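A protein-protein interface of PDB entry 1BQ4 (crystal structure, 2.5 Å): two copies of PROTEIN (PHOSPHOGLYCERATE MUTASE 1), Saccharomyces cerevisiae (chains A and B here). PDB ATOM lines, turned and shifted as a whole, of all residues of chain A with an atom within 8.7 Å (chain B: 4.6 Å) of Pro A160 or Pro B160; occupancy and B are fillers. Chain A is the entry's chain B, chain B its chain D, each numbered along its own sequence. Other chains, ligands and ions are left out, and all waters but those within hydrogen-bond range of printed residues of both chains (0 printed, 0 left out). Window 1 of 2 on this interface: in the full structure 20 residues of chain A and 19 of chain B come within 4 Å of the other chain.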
ATOM      1  N   SER A  81      -3.814 -15.345 -11.618  1.00  0.00           N
ATOM      2  CA  SER A  81      -3.150 -14.214 -11.047  1.00  0.00           C
ATOM      3  C   SER A  81      -1.696 -14.343 -11.323  1.00  0.00           C
ATOM      4  O   SER A  81      -1.168 -15.449 -11.311  1.00  0.00           O
ATOM      5  CB  SER A  81      -3.369 -14.155  -9.533  1.00  0.00           C
ATOM      6  OG  SER A  81      -2.501 -13.222  -8.924  1.00  0.00           O
ATOM      7  N   TRP A  82      -1.052 -13.194 -11.499  1.00  0.00           N
ATOM      8  CA  TRP A  82       0.375 -13.144 -11.743  1.00  0.00           C
ATOM      9  C   TRP A  82       1.090 -13.585 -10.484  1.00  0.00           C
ATOM     10  O   TRP A  82       2.247 -13.968 -10.549  1.00  0.00           O
ATOM     11  CB  TRP A  82       0.825 -11.726 -12.108  1.00  0.00           C
ATOM     12  CG  TRP A  82       0.881 -10.742 -10.935  1.00  0.00           C
ATOM     13  CD1 TRP A  82      -0.144 -10.037 -10.420  1.00  0.00           C
ATOM     14  CD2 TRP A  82       2.041 -10.354 -10.184  1.00  0.00           C
ATOM     15  NE1 TRP A  82       0.281  -9.240  -9.403  1.00  0.00           N
ATOM     16  CE2 TRP A  82       1.622  -9.415  -9.228  1.00  0.00           C
ATOM     17  CE3 TRP A  82       3.404 -10.711 -10.226  1.00  0.00           C
ATOM     18  CZ2 TRP A  82       2.507  -8.829  -8.312  1.00  0.00           C
ATOM     19  CZ3 TRP A  82       4.290 -10.125  -9.326  1.00  0.00           C
ATOM     20  CH2 TRP A  82       3.842  -9.202  -8.383  1.00  0.00           C
ATOM     21  N   ARG A  83       0.399 -13.523  -9.346  1.00  0.00           N
ATOM     22  CA  ARG A  83       0.981 -13.897  -8.053  1.00  0.00           C
ATOM     23  C   ARG A  83       1.227 -15.375  -7.859  1.00  0.00           C
ATOM     24  O   ARG A  83       1.866 -15.781  -6.881  1.00  0.00           O
ATOM     25  CB  ARG A  83       0.159 -13.325  -6.902  1.00  0.00           C
ATOM     26  CG  ARG A  83       0.126 -11.828  -6.943  1.00  0.00           C
ATOM     27  CD  ARG A  83      -0.748 -11.202  -5.836  1.00  0.00           C
ATOM     28  NE  ARG A  83      -0.747  -9.734  -5.951  1.00  0.00           N
ATOM     29  CZ  ARG A  83       0.020  -8.916  -5.228  1.00  0.00           C
ATOM     30  NH1 ARG A  83       0.818  -9.404  -4.287  1.00  0.00           N
ATOM     31  NH2 ARG A  83       0.174  -7.644  -5.588  1.00  0.00           N
ATOM     32  N   VAL A 140      -2.581  -4.346 -13.750  1.00  0.00           N
ATOM     33  CA  VAL A 140      -1.832  -4.466 -12.497  1.00  0.00           C
ATOM     34  C   VAL A 140      -0.927  -3.245 -12.438  1.00  0.00           C
ATOM     35  O   VAL A 140      -0.519  -2.747 -13.490  1.00  0.00           O
ATOM     36  CB  VAL A 140      -0.928  -5.733 -12.472  1.00  0.00           C
ATOM     37  CG1 VAL A 140      -0.217  -5.842 -11.148  1.00  0.00           C
ATOM     38  CG2 VAL A 140      -1.755  -6.984 -12.680  1.00  0.00           C
ATOM     39  N   ASP A 141      -0.675  -2.733 -11.226  1.00  0.00           N
ATOM     40  CA  ASP A 141       0.204  -1.576 -10.995  1.00  0.00           C
ATOM     41  C   ASP A 141       1.533  -1.831 -11.720  1.00  0.00           C
ATOM     42  O   ASP A 141       2.321  -2.681 -11.304  1.00  0.00           O
ATOM     43  CB  ASP A 141       0.432  -1.395  -9.459  1.00  0.00           C
ATOM     44  CG  ASP A 141       1.426  -0.238  -9.075  1.00  0.00           C
ATOM     45  OD1 ASP A 141       1.911   0.584  -9.909  1.00  0.00           O
ATOM     46  OD2 ASP A 141       1.725  -0.145  -7.860  1.00  0.00           O
ATOM     47  N   VAL A 144       4.749  -2.676  -9.661  1.00  0.00           N
ATOM     48  CA  VAL A 144       5.027  -3.920  -8.946  1.00  0.00           C
ATOM     49  C   VAL A 144       5.573  -5.150  -9.744  1.00  0.00           C
ATOM     50  O   VAL A 144       6.133  -6.114  -9.149  1.00  0.00           O
ATOM     51  CB  VAL A 144       3.826  -4.314  -8.065  1.00  0.00           C
ATOM     52  CG1 VAL A 144       2.636  -4.966  -8.896  1.00  0.00           C
ATOM     53  CG2 VAL A 144       4.308  -5.246  -6.961  1.00  0.00           C
ATOM     54  N   LEU A 153      11.130 -13.126  -2.597  1.00  0.00           N
ATOM     55  CA  LEU A 153      10.283 -12.155  -3.255  1.00  0.00           C
ATOM     56  C   LEU A 153       9.017 -12.758  -3.736  1.00  0.00           C
ATOM     57  O   LEU A 153       7.915 -12.240  -3.416  1.00  0.00           O
ATOM     58  CB  LEU A 153      11.046 -11.457  -4.394  1.00  0.00           C
ATOM     59  CG  LEU A 153      11.873 -10.191  -3.996  1.00  0.00           C
ATOM     60  CD1 LEU A 153      12.388 -10.281  -2.562  1.00  0.00           C
ATOM     61  CD2 LEU A 153      13.047  -9.936  -4.959  1.00  0.00           C
ATOM     62  N   VAL A 154       9.158 -13.870  -4.470  1.00  0.00           N
ATOM     63  CA  VAL A 154       8.009 -14.584  -5.005  1.00  0.00           C
ATOM     64  C   VAL A 154       6.998 -14.723  -3.910  1.00  0.00           C
ATOM     65  O   VAL A 154       5.834 -14.470  -4.148  1.00  0.00           O
ATOM     66  CB  VAL A 154       8.348 -16.010  -5.553  1.00  0.00           C
ATOM     67  CG1 VAL A 154       7.065 -16.875  -5.736  1.00  0.00           C
ATOM     68  CG2 VAL A 154       8.994 -15.868  -6.880  1.00  0.00           C
ATOM     69  N   ILE A 155       7.443 -15.065  -2.700  1.00  0.00           N
ATOM     70  CA  ILE A 155       6.522 -15.236  -1.581  1.00  0.00           C
ATOM     71  C   ILE A 155       5.975 -13.856  -1.124  1.00  0.00           C
ATOM     72  O   ILE A 155       4.760 -13.726  -0.854  1.00  0.00           O
ATOM     73  CB  ILE A 155       7.206 -15.937  -0.388  1.00  0.00           C
ATOM     74  CG1 ILE A 155       7.853 -17.251  -0.831  1.00  0.00           C
ATOM     75  CG2 ILE A 155       6.209 -16.086   0.778  1.00  0.00           C
ATOM     76  CD1 ILE A 155       8.707 -17.970   0.245  1.00  0.00           C
ATOM     77  N   ASP A 156       6.828 -12.823  -1.055  1.00  0.00           N
ATOM     78  CA  ASP A 156       6.344 -11.503  -0.643  1.00  0.00           C
ATOM     79  C   ASP A 156       5.097 -11.162  -1.473  1.00  0.00           C
ATOM     80  O   ASP A 156       4.152 -10.595  -0.939  1.00  0.00           O
ATOM     81  CB  ASP A 156       7.422 -10.395  -0.830  1.00  0.00           C
ATOM     82  CG  ASP A 156       8.598 -10.521   0.146  1.00  0.00           C
ATOM     83  OD1 ASP A 156       9.555  -9.684   0.079  1.00  0.00           O
ATOM     84  OD2 ASP A 156       8.577 -11.463   0.976  1.00  0.00           O
ATOM     85  N   ARG A 157       5.102 -11.534  -2.762  1.00  0.00           N
ATOM     86  CA  ARG A 157       3.980 -11.266  -3.719  1.00  0.00           C
ATOM     87  C   ARG A 157       2.856 -12.300  -3.859  1.00  0.00           C
ATOM     88  O   ARG A 157       1.782 -11.969  -4.343  1.00  0.00           O
ATOM     89  CB  ARG A 157       4.504 -10.922  -5.135  1.00  0.00           C
ATOM     90  CG  ARG A 157       5.564 -11.896  -5.714  1.00  0.00           C
ATOM     91  CD  ARG A 157       5.234 -12.434  -7.116  1.00  0.00           C
ATOM     92  NE  ARG A 157       4.891 -13.848  -7.104  1.00  0.00           N
ATOM     93  CZ  ARG A 157       5.153 -14.697  -8.095  1.00  0.00           C
ATOM     94  NH1 ARG A 157       5.770 -14.272  -9.194  1.00  0.00           N
ATOM     95  NH2 ARG A 157       4.803 -15.969  -7.980  1.00  0.00           N
ATOM     96  N   LEU A 158       3.106 -13.557  -3.506  1.00  0.00           N
ATOM     97  CA  LEU A 158       2.058 -14.576  -3.606  1.00  0.00           C
ATOM     98  C   LEU A 158       1.141 -14.474  -2.415  1.00  0.00           C
ATOM     99  O   LEU A 158      -0.078 -14.540  -2.557  1.00  0.00           O
ATOM    100  CB  LEU A 158       2.672 -15.996  -3.716  1.00  0.00           C
ATOM    101  CG  LEU A 158       1.853 -17.257  -3.402  1.00  0.00           C
ATOM    102  CD1 LEU A 158       2.289 -18.414  -4.304  1.00  0.00           C
ATOM    103  CD2 LEU A 158       2.014 -17.626  -1.915  1.00  0.00           C
ATOM    104  N   LEU A 159       1.741 -14.359  -1.236  1.00  0.00           N
ATOM    105  CA  LEU A 159       0.987 -14.250   0.018  1.00  0.00           C
ATOM    106  C   LEU A 159      -0.324 -13.425   0.049  1.00  0.00           C
ATOM    107  O   LEU A 159      -1.309 -13.887   0.630  1.00  0.00           O
ATOM    108  CB  LEU A 159       1.903 -13.809   1.167  1.00  0.00           C
ATOM    109  CG  LEU A 159       2.847 -14.870   1.720  1.00  0.00           C
ATOM    110  CD1 LEU A 159       3.448 -14.390   2.995  1.00  0.00           C
ATOM    111  CD2 LEU A 159       2.091 -16.169   1.977  1.00  0.00           C
ATOM    112  N   PRO A 160      -0.344 -12.186  -0.507  1.00  0.00           N
ATOM    113  CA  PRO A 160      -1.553 -11.324  -0.518  1.00  0.00           C
ATOM    114  C   PRO A 160      -2.799 -11.843  -1.291  1.00  0.00           C
ATOM    115  O   PRO A 160      -3.938 -11.441  -1.056  1.00  0.00           O
ATOM    116  CB  PRO A 160      -1.018 -10.010  -1.111  1.00  0.00           C
ATOM    117  CG  PRO A 160       0.432  -9.979  -0.701  1.00  0.00           C
ATOM    118  CD  PRO A 160       0.850 -11.418  -0.926  1.00  0.00           C
ATOM    119  N   TYR A 161      -2.548 -12.717  -2.251  1.00  0.00           N
ATOM    120  CA  TYR A 161      -3.577 -13.339  -3.063  1.00  0.00           C
ATOM    121  C   TYR A 161      -4.054 -14.531  -2.286  1.00  0.00           C
ATOM    122  O   TYR A 161      -5.175 -14.979  -2.419  1.00  0.00           O
ATOM    123  CB  TYR A 161      -2.941 -13.793  -4.369  1.00  0.00           C
ATOM    124  CG  TYR A 161      -3.926 -14.241  -5.403  1.00  0.00           C
ATOM    125  CD1 TYR A 161      -4.811 -13.348  -5.990  1.00  0.00           C
ATOM    126  CD2 TYR A 161      -4.005 -15.577  -5.766  1.00  0.00           C
ATOM    127  CE1 TYR A 161      -5.770 -13.801  -6.925  1.00  0.00           C
ATOM    128  CE2 TYR A 161      -4.942 -16.034  -6.670  1.00  0.00           C
ATOM    129  CZ  TYR A 161      -5.825 -15.153  -7.243  1.00  0.00           C
ATOM    130  OH  TYR A 161      -6.796 -15.650  -8.068  1.00  0.00           O
ATOM    131  N   TRP A 162      -3.167 -15.095  -1.505  1.00  0.00           N
ATOM    132  CA  TRP A 162      -3.504 -16.256  -0.714  1.00  0.00           C
ATOM    133  C   TRP A 162      -4.307 -15.786   0.482  1.00  0.00           C
ATOM    134  O   TRP A 162      -5.371 -16.336   0.793  1.00  0.00           O
ATOM    135  CB  TRP A 162      -2.210 -16.972  -0.295  1.00  0.00           C
ATOM    136  CG  TRP A 162      -2.300 -17.822   0.942  1.00  0.00           C
ATOM    137  CD1 TRP A 162      -1.864 -17.498   2.214  1.00  0.00           C
ATOM    138  CD2 TRP A 162      -2.849 -19.137   1.032  1.00  0.00           C
ATOM    139  NE1 TRP A 162      -2.118 -18.529   3.079  1.00  0.00           N
ATOM    140  CE2 TRP A 162      -2.730 -19.546   2.387  1.00  0.00           C
ATOM    141  CE3 TRP A 162      -3.415 -20.023   0.104  1.00  0.00           C
ATOM    142  CZ2 TRP A 162      -3.172 -20.812   2.827  1.00  0.00           C
ATOM    143  CZ3 TRP A 162      -3.844 -21.277   0.538  1.00  0.00           C
ATOM    144  CH2 TRP A 162      -3.722 -21.660   1.882  1.00  0.00           C
ATOM    145  N   GLN A 163      -3.858 -14.688   1.064  1.00  0.00           N
ATOM    146  CA  GLN A 163      -4.486 -14.141   2.244  1.00  0.00           C
ATOM    147  C   GLN A 163      -5.949 -13.674   2.068  1.00  0.00           C
ATOM    148  O   GLN A 163      -6.797 -13.941   2.923  1.00  0.00           O
ATOM    149  CB  GLN A 163      -3.609 -12.979   2.781  1.00  0.00           C
ATOM    150  CG  GLN A 163      -2.234 -13.414   3.255  1.00  0.00           C
ATOM    151  CD  GLN A 163      -1.248 -12.264   3.523  1.00  0.00           C
ATOM    152  OE1 GLN A 163      -1.229 -11.239   2.833  1.00  0.00           O
ATOM    153  NE2 GLN A 163      -0.375 -12.478   4.493  1.00  0.00           N
ATOM    154  N   ASP A 164      -6.240 -13.075   0.909  1.00  0.00           N
ATOM    155  CA  ASP A 164      -7.523 -12.467   0.599  1.00  0.00           C
ATOM    156  C   ASP A 164      -8.445 -13.203  -0.293  1.00  0.00           C
ATOM    157  O   ASP A 164      -9.670 -13.042  -0.187  1.00  0.00           O
ATOM    158  CB  ASP A 164      -7.290 -11.158  -0.155  1.00  0.00           C
ATOM    159  CG  ASP A 164      -6.814 -10.027   0.710  1.00  0.00           C
ATOM    160  OD1 ASP A 164      -6.768  -8.925   0.138  1.00  0.00           O
ATOM    161  OD2 ASP A 164      -6.500 -10.216   1.910  1.00  0.00           O
ATOM    162  N   VAL A 165      -7.830 -13.711  -1.352  1.00  0.00           N
ATOM    163  CA  VAL A 165      -8.528 -14.392  -2.440  1.00  0.00           C
ATOM    164  C   VAL A 165      -8.780 -15.901  -2.391  1.00  0.00           C
ATOM    165  O   VAL A 165      -9.933 -16.346  -2.478  1.00  0.00           O
ATOM    166  CB  VAL A 165      -7.894 -13.971  -3.789  1.00  0.00           C
ATOM    167  CG1 VAL A 165      -8.719 -14.493  -4.944  1.00  0.00           C
ATOM    168  CG2 VAL A 165      -7.798 -12.401  -3.851  1.00  0.00           C
ATOM    169  N   ILE A 166      -7.697 -16.665  -2.308  1.00  0.00           N
ATOM    170  CA  ILE A 166      -7.720 -18.119  -2.224  1.00  0.00           C
ATOM    171  C   ILE A 166      -8.212 -18.542  -0.832  1.00  0.00           C
ATOM    172  O   ILE A 166      -8.628 -19.679  -0.644  1.00  0.00           O
ATOM    173  CB  ILE A 166      -6.288 -18.683  -2.414  1.00  0.00           C
ATOM    174  CG1 ILE A 166      -5.743 -18.333  -3.790  1.00  0.00           C
ATOM    175  CG2 ILE A 166      -6.231 -20.161  -2.172  1.00  0.00           C
ATOM    176  CD1 ILE A 166      -4.361 -18.842  -4.022  1.00  0.00           C
ATOM    177  N   ALA A 167      -8.106 -17.669   0.166  1.00  0.00           N
ATOM    178  CA  ALA A 167      -8.558 -18.034   1.507  1.00  0.00           C
ATOM    179  C   ALA A 167     -10.055 -17.914   1.727  1.00  0.00           C
ATOM    180  O   ALA A 167     -10.597 -18.689   2.516  1.00  0.00           O
ATOM    181  CB  ALA A 167      -7.816 -17.296   2.550  1.00  0.00           C
ATOM    182  N   HIS A 191       5.326 -21.366   3.534  1.00  0.00           N
ATOM    183  CA  HIS A 191       4.466 -20.535   4.372  1.00  0.00           C
ATOM    184  C   HIS A 191       3.652 -21.512   5.188  1.00  0.00           C
ATOM    185  O   HIS A 191       3.619 -21.426   6.416  1.00  0.00           O
ATOM    186  CB  HIS A 191       3.533 -19.675   3.506  1.00  0.00           C
ATOM    187  CG  HIS A 191       2.608 -18.789   4.299  1.00  0.00           C
ATOM    188  ND1 HIS A 191       3.028 -17.634   4.925  1.00  0.00           N
ATOM    189  CD2 HIS A 191       1.292 -18.918   4.595  1.00  0.00           C
ATOM    190  CE1 HIS A 191       2.013 -17.100   5.575  1.00  0.00           C
ATOM    191  NE2 HIS A 191       0.948 -17.858   5.393  1.00  0.00           N
ATOM    192  N   ARG B  83      -7.639  -4.123   4.294  1.00  0.00           N
ATOM    193  CA  ARG B  83      -6.317  -3.563   4.003  1.00  0.00           C
ATOM    194  C   ARG B  83      -6.372  -2.070   3.864  1.00  0.00           C
ATOM    195  O   ARG B  83      -5.342  -1.411   3.818  1.00  0.00           O
ATOM    196  CB  ARG B  83      -5.750  -4.178   2.736  1.00  0.00           C
ATOM    197  CG  ARG B  83      -5.595  -5.681   2.797  1.00  0.00           C
ATOM    198  CD  ARG B  83      -4.980  -6.180   1.490  1.00  0.00           C
ATOM    199  NE  ARG B  83      -4.825  -7.631   1.487  1.00  0.00           N
ATOM    200  CZ  ARG B  83      -3.736  -8.296   1.895  1.00  0.00           C
ATOM    201  NH1 ARG B  83      -2.639  -7.649   2.353  1.00  0.00           N
ATOM    202  NH2 ARG B  83      -3.793  -9.627   1.918  1.00  0.00           N
ATOM    203  N   ASP B 156       2.491  -2.045   3.836  1.00  0.00           N
ATOM    204  CA  ASP B 156       2.822  -3.392   3.364  1.00  0.00           C
ATOM    205  C   ASP B 156       1.613  -4.255   3.114  1.00  0.00           C
ATOM    206  O   ASP B 156       1.603  -5.046   2.179  1.00  0.00           O
ATOM    207  CB  ASP B 156       3.795  -4.112   4.317  1.00  0.00           C
ATOM    208  CG  ASP B 156       5.176  -3.456   4.371  1.00  0.00           C
ATOM    209  OD1 ASP B 156       5.887  -3.714   5.363  1.00  0.00           O
ATOM    210  OD2 ASP B 156       5.543  -2.662   3.456  1.00  0.00           O
ATOM    211  N   ARG B 157       0.608  -4.123   3.969  1.00  0.00           N
ATOM    212  CA  ARG B 157      -0.617  -4.895   3.823  1.00  0.00           C
ATOM    213  C   ARG B 157      -1.564  -4.249   2.830  1.00  0.00           C
ATOM    214  O   ARG B 157      -2.326  -4.934   2.157  1.00  0.00           O
ATOM    215  CB  ARG B 157      -1.288  -5.097   5.178  1.00  0.00           C
ATOM    216  CG  ARG B 157      -1.429  -3.841   6.039  1.00  0.00           C
ATOM    217  CD  ARG B 157      -2.773  -3.164   5.849  1.00  0.00           C
ATOM    218  NE  ARG B 157      -3.280  -2.706   7.126  1.00  0.00           N
ATOM    219  CZ  ARG B 157      -4.086  -1.663   7.282  1.00  0.00           C
ATOM    220  NH1 ARG B 157      -4.502  -0.985   6.221  1.00  0.00           N
ATOM    221  NH2 ARG B 157      -4.334  -1.186   8.506  1.00  0.00           N
ATOM    222  N   LEU B 158      -1.422  -2.938   2.673  1.00  0.00           N
ATOM    223  CA  LEU B 158      -2.259  -2.140   1.769  1.00  0.00           C
ATOM    224  C   LEU B 158      -1.889  -2.214   0.289  1.00  0.00           C
ATOM    225  O   LEU B 158      -2.742  -2.476  -0.562  1.00  0.00           O
ATOM    226  CB  LEU B 158      -2.264  -0.664   2.226  1.00  0.00           C
ATOM    227  CG  LEU B 158      -3.102   0.312   1.380  1.00  0.00           C
ATOM    228  CD1 LEU B 158      -3.967   1.172   2.313  1.00  0.00           C
ATOM    229  CD2 LEU B 158      -2.234   1.188   0.480  1.00  0.00           C
ATOM    230  N   LEU B 159      -0.611  -1.992   0.003  1.00  0.00           N
ATOM    231  CA  LEU B 159      -0.080  -1.988  -1.355  1.00  0.00           C
ATOM    232  C   LEU B 159      -0.660  -3.025  -2.329  1.00  0.00           C
ATOM    233  O   LEU B 159      -1.092  -2.649  -3.424  1.00  0.00           O
ATOM    234  CB  LEU B 159       1.448  -2.061  -1.339  1.00  0.00           C
ATOM    235  CG  LEU B 159       2.217  -0.814  -0.947  1.00  0.00           C
ATOM    236  CD1 LEU B 159       3.699  -0.973  -1.336  1.00  0.00           C
ATOM    237  CD2 LEU B 159       1.602   0.345  -1.679  1.00  0.00           C
ATOM    238  N   PRO B 160      -0.687  -4.332  -1.955  1.00  0.00           N
ATOM    239  CA  PRO B 160      -1.207  -5.442  -2.781  1.00  0.00           C
ATOM    240  C   PRO B 160      -2.651  -5.290  -3.282  1.00  0.00           C
ATOM    241  O   PRO B 160      -3.008  -5.866  -4.298  1.00  0.00           O
ATOM    242  CB  PRO B 160      -1.080  -6.646  -1.834  1.00  0.00           C
ATOM    243  CG  PRO B 160       0.083  -6.285  -0.980  1.00  0.00           C
ATOM    244  CD  PRO B 160      -0.200  -4.857  -0.666  1.00  0.00           C
ATOM    245  N   TYR B 161      -3.488  -4.582  -2.511  1.00  0.00           N
ATOM    246  CA  TYR B 161      -4.890  -4.289  -2.847  1.00  0.00           C
ATOM    247  C   TYR B 161      -4.888  -3.112  -3.833  1.00  0.00           C
ATOM    248  O   TYR B 161      -5.737  -3.016  -4.686  1.00  0.00           O
ATOM    249  CB  TYR B 161      -5.628  -3.916  -1.572  1.00  0.00           C
ATOM    250  CG  TYR B 161      -7.115  -3.829  -1.726  1.00  0.00           C
ATOM    251  CD1 TYR B 161      -7.844  -4.942  -2.058  1.00  0.00           C
ATOM    252  CD2 TYR B 161      -7.803  -2.598  -1.562  1.00  0.00           C
ATOM    253  CE1 TYR B 161      -9.222  -4.858  -2.242  1.00  0.00           C
ATOM    254  CE2 TYR B 161      -9.190  -2.499  -1.737  1.00  0.00           C
ATOM    255  CZ  TYR B 161      -9.881  -3.638  -2.082  1.00  0.00           C
ATOM    256  OH  TYR B 161     -11.230  -3.607  -2.302  1.00  0.00           O
ATOM    257  N   TRP B 162      -3.947  -2.192  -3.669  1.00  0.00           N
ATOM    258  CA  TRP B 162      -3.764  -1.042  -4.577  1.00  0.00           C
ATOM    259  C   TRP B 162      -3.258  -1.566  -5.941  1.00  0.00           C
ATOM    260  O   TRP B 162      -3.800  -1.237  -7.015  1.00  0.00           O
ATOM    261  CB  TRP B 162      -2.690  -0.091  -3.986  1.00  0.00           C
ATOM    262  CG  TRP B 162      -2.156   0.978  -4.945  1.00  0.00           C
ATOM    263  CD1 TRP B 162      -0.979   0.935  -5.623  1.00  0.00           C
ATOM    264  CD2 TRP B 162      -2.858   2.147  -5.427  1.00  0.00           C
ATOM    265  NE1 TRP B 162      -0.923   1.960  -6.528  1.00  0.00           N
ATOM    266  CE2 TRP B 162      -2.064   2.715  -6.434  1.00  0.00           C
ATOM    267  CE3 TRP B 162      -4.086   2.770  -5.092  1.00  0.00           C
ATOM    268  CZ2 TRP B 162      -2.451   3.866  -7.126  1.00  0.00           C
ATOM    269  CZ3 TRP B 162      -4.468   3.922  -5.779  1.00  0.00           C
ATOM    270  CH2 TRP B 162      -3.648   4.454  -6.792  1.00  0.00           C
ATOM    271  N   GLN B 163      -2.184  -2.353  -5.858  1.00  0.00           N
ATOM    272  CA  GLN B 163      -1.503  -2.994  -6.970  1.00  0.00           C
ATOM    273  C   GLN B 163      -2.434  -3.783  -7.857  1.00  0.00           C
ATOM    274  O   GLN B 163      -2.487  -3.522  -9.065  1.00  0.00           O
ATOM    275  CB  GLN B 163      -0.399  -3.888  -6.413  1.00  0.00           C
ATOM    276  CG  GLN B 163       0.875  -3.096  -6.162  1.00  0.00           C
ATOM    277  CD  GLN B 163       1.817  -3.656  -5.100  1.00  0.00           C
ATOM    278  OE1 GLN B 163       1.630  -4.762  -4.586  1.00  0.00           O
ATOM    279  NE2 GLN B 163       2.867  -2.876  -4.778  1.00  0.00           N
ATOM    280  N   ASP B 164      -3.208  -4.692  -7.251  1.00  0.00           N
ATOM    281  CA  ASP B 164      -4.144  -5.579  -7.961  1.00  0.00           C
ATOM    282  C   ASP B 164      -5.581  -5.127  -8.116  1.00  0.00           C
ATOM    283  O   ASP B 164      -6.179  -5.251  -9.186  1.00  0.00           O
ATOM    284  CB  ASP B 164      -4.192  -6.945  -7.270  1.00  0.00           C
ATOM    285  CG  ASP B 164      -2.971  -7.771  -7.528  1.00  0.00           C
ATOM    286  OD1 ASP B 164      -2.979  -8.946  -7.128  1.00  0.00           O
ATOM    287  OD2 ASP B 164      -2.003  -7.251  -8.132  1.00  0.00           O
ATOM    288  N   VAL B 165      -6.167  -4.685  -7.023  1.00  0.00           N
ATOM    289  CA  VAL B 165      -7.555  -4.294  -7.056  1.00  0.00           C
ATOM    290  C   VAL B 165      -7.908  -2.833  -7.368  1.00  0.00           C
ATOM    291  O   VAL B 165      -8.666  -2.582  -8.316  1.00  0.00           O
ATOM    292  CB  VAL B 165      -8.272  -4.873  -5.805  1.00  0.00           C
ATOM    293  CG1 VAL B 165      -9.813  -4.919  -6.038  1.00  0.00           C
ATOM    294  CG2 VAL B 165      -7.694  -6.350  -5.512  1.00  0.00           C
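The backbone carbonyl oxygen of Pro A160 sits at hydrogen-bond distance from the guanidinium group of Arg B83.
NH2 of Arg B83 lies within hydrogen-bond range of OE1 of Gln A163, 3.2 Å away.
The guanidinium group (NE) of Arg B83 is in salt-bridge range of the side-chain carboxylate (OD1) of Asp A164.
OE1 of Gln B163 lies within hydrogen-bond range of NH2 of Arg A83 (3.4 Å).
The backbone carbonyl oxygen (O) of Gln B163 is in hydrogen-bond range of the backbone NH (N) of Asp A141 (2.9 Å).
The side-chain carboxylate (OD2) of Asp B164 sits at hydrogen-bond distance from the indole nitrogen (NE1) of Trp A82, 3.3 Å away.
The side-chain carboxylate of Asp B164 is in salt-bridge range of the guanidinium group of Arg A83.
Printed residues of chain B within 4 Å of Arg A83: Pro B160 (3.8 Å), Gln B163 (3.4 Å) and Asp B164 (2.6 Å).
Printed residues of chain B within 4 Å of Val A144: Gln B163.
Of chain B, only Arg B83 (3.5 Å) and Pro B160 (3.4 Å) come within 4 Å of Pro A160.
Trp A162 touches none of the printed residues of chain B.
Of chain A, only Arg A83 (3.8 Å) and Pro A160 (3.4 Å) come within 4 Å of Pro B160.
The nearest residue of chain A that does not touch Pro B160 is Asp A156 (5.9 Å).
The nearest printed residue of chain B that does not touch Arg A83 is Leu B159 (5.6 Å).
The backbone carbonyl oxygen of Arg B83 is in hydrogen-bond range of the guanidinium group of Arg B157 (2.6 Å).
The backbone NH (N) of Arg A83 is in hydrogen-bond range of the side-chain hydroxyl (OG) of Ser A81 (2.9 Å).
The guanidinium group (NH1) of Arg A83 lies within hydrogen-bond range of the backbone carbonyl oxygen (O) of Arg A157, at 2.7 Å.
The backbone carbonyl oxygen (O) of Leu A159 lies close to the side-chain amide oxygen (OE1) of Gln A163, at 3.4 Å.
Of the 22 printed residues of chain A, 8 touch a printed residue of chain B.
Printed residues of chain A that touch a printed residue of chain B: Trp A82, Arg A83, Val A140, Asp A141, Val A144, Pro A160, Gln A163 and Asp A164.
Along chain A the printed residues that touch a printed residue of chain B span positions 82 to 164.
Hydrophobic or aromatic side chains of chain B that line the printed part of chain A: Pro B160 and Trp B162.
Among the printed residues, 13 pairs touch across the chains.
Among the printed residues, Asp or Glu carboxylates within 4 Å of a Lys or Arg side-chain nitrogen of the other chain: Arg A83 with Asp B164 (2.6 Å) and Asp A164 with Arg B83 (2.7 Å).
Pro B160 touches Arg A83 (CA to NH2, 3.8 Å).
Val A140 touches Gln B163 (CA to O, 3.6 Å).
Val A140 touches Asp B164.
NE1 of Trp B162 touches OD2 of Asp A141, at 3.6 Å.
Val A144 touches Gln B163.
Pro B160 touches Pro A160.
Arg A83 touches Pro B160, and with the chains exchanged Pro A160 touches Arg B83.
Arg A83 touches Gln B163, and with the chains exchanged Gln A163 touches Arg B83.
Arg A83 touches Asp B164, and with the chains exchanged Asp A164 touches Arg B83.
Pro A160 touches its own counterpart, Pro B160.
Of the 13 pairs that touch across the chains among the printed residues, 7 have their exchanged pair printed and touching as well.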
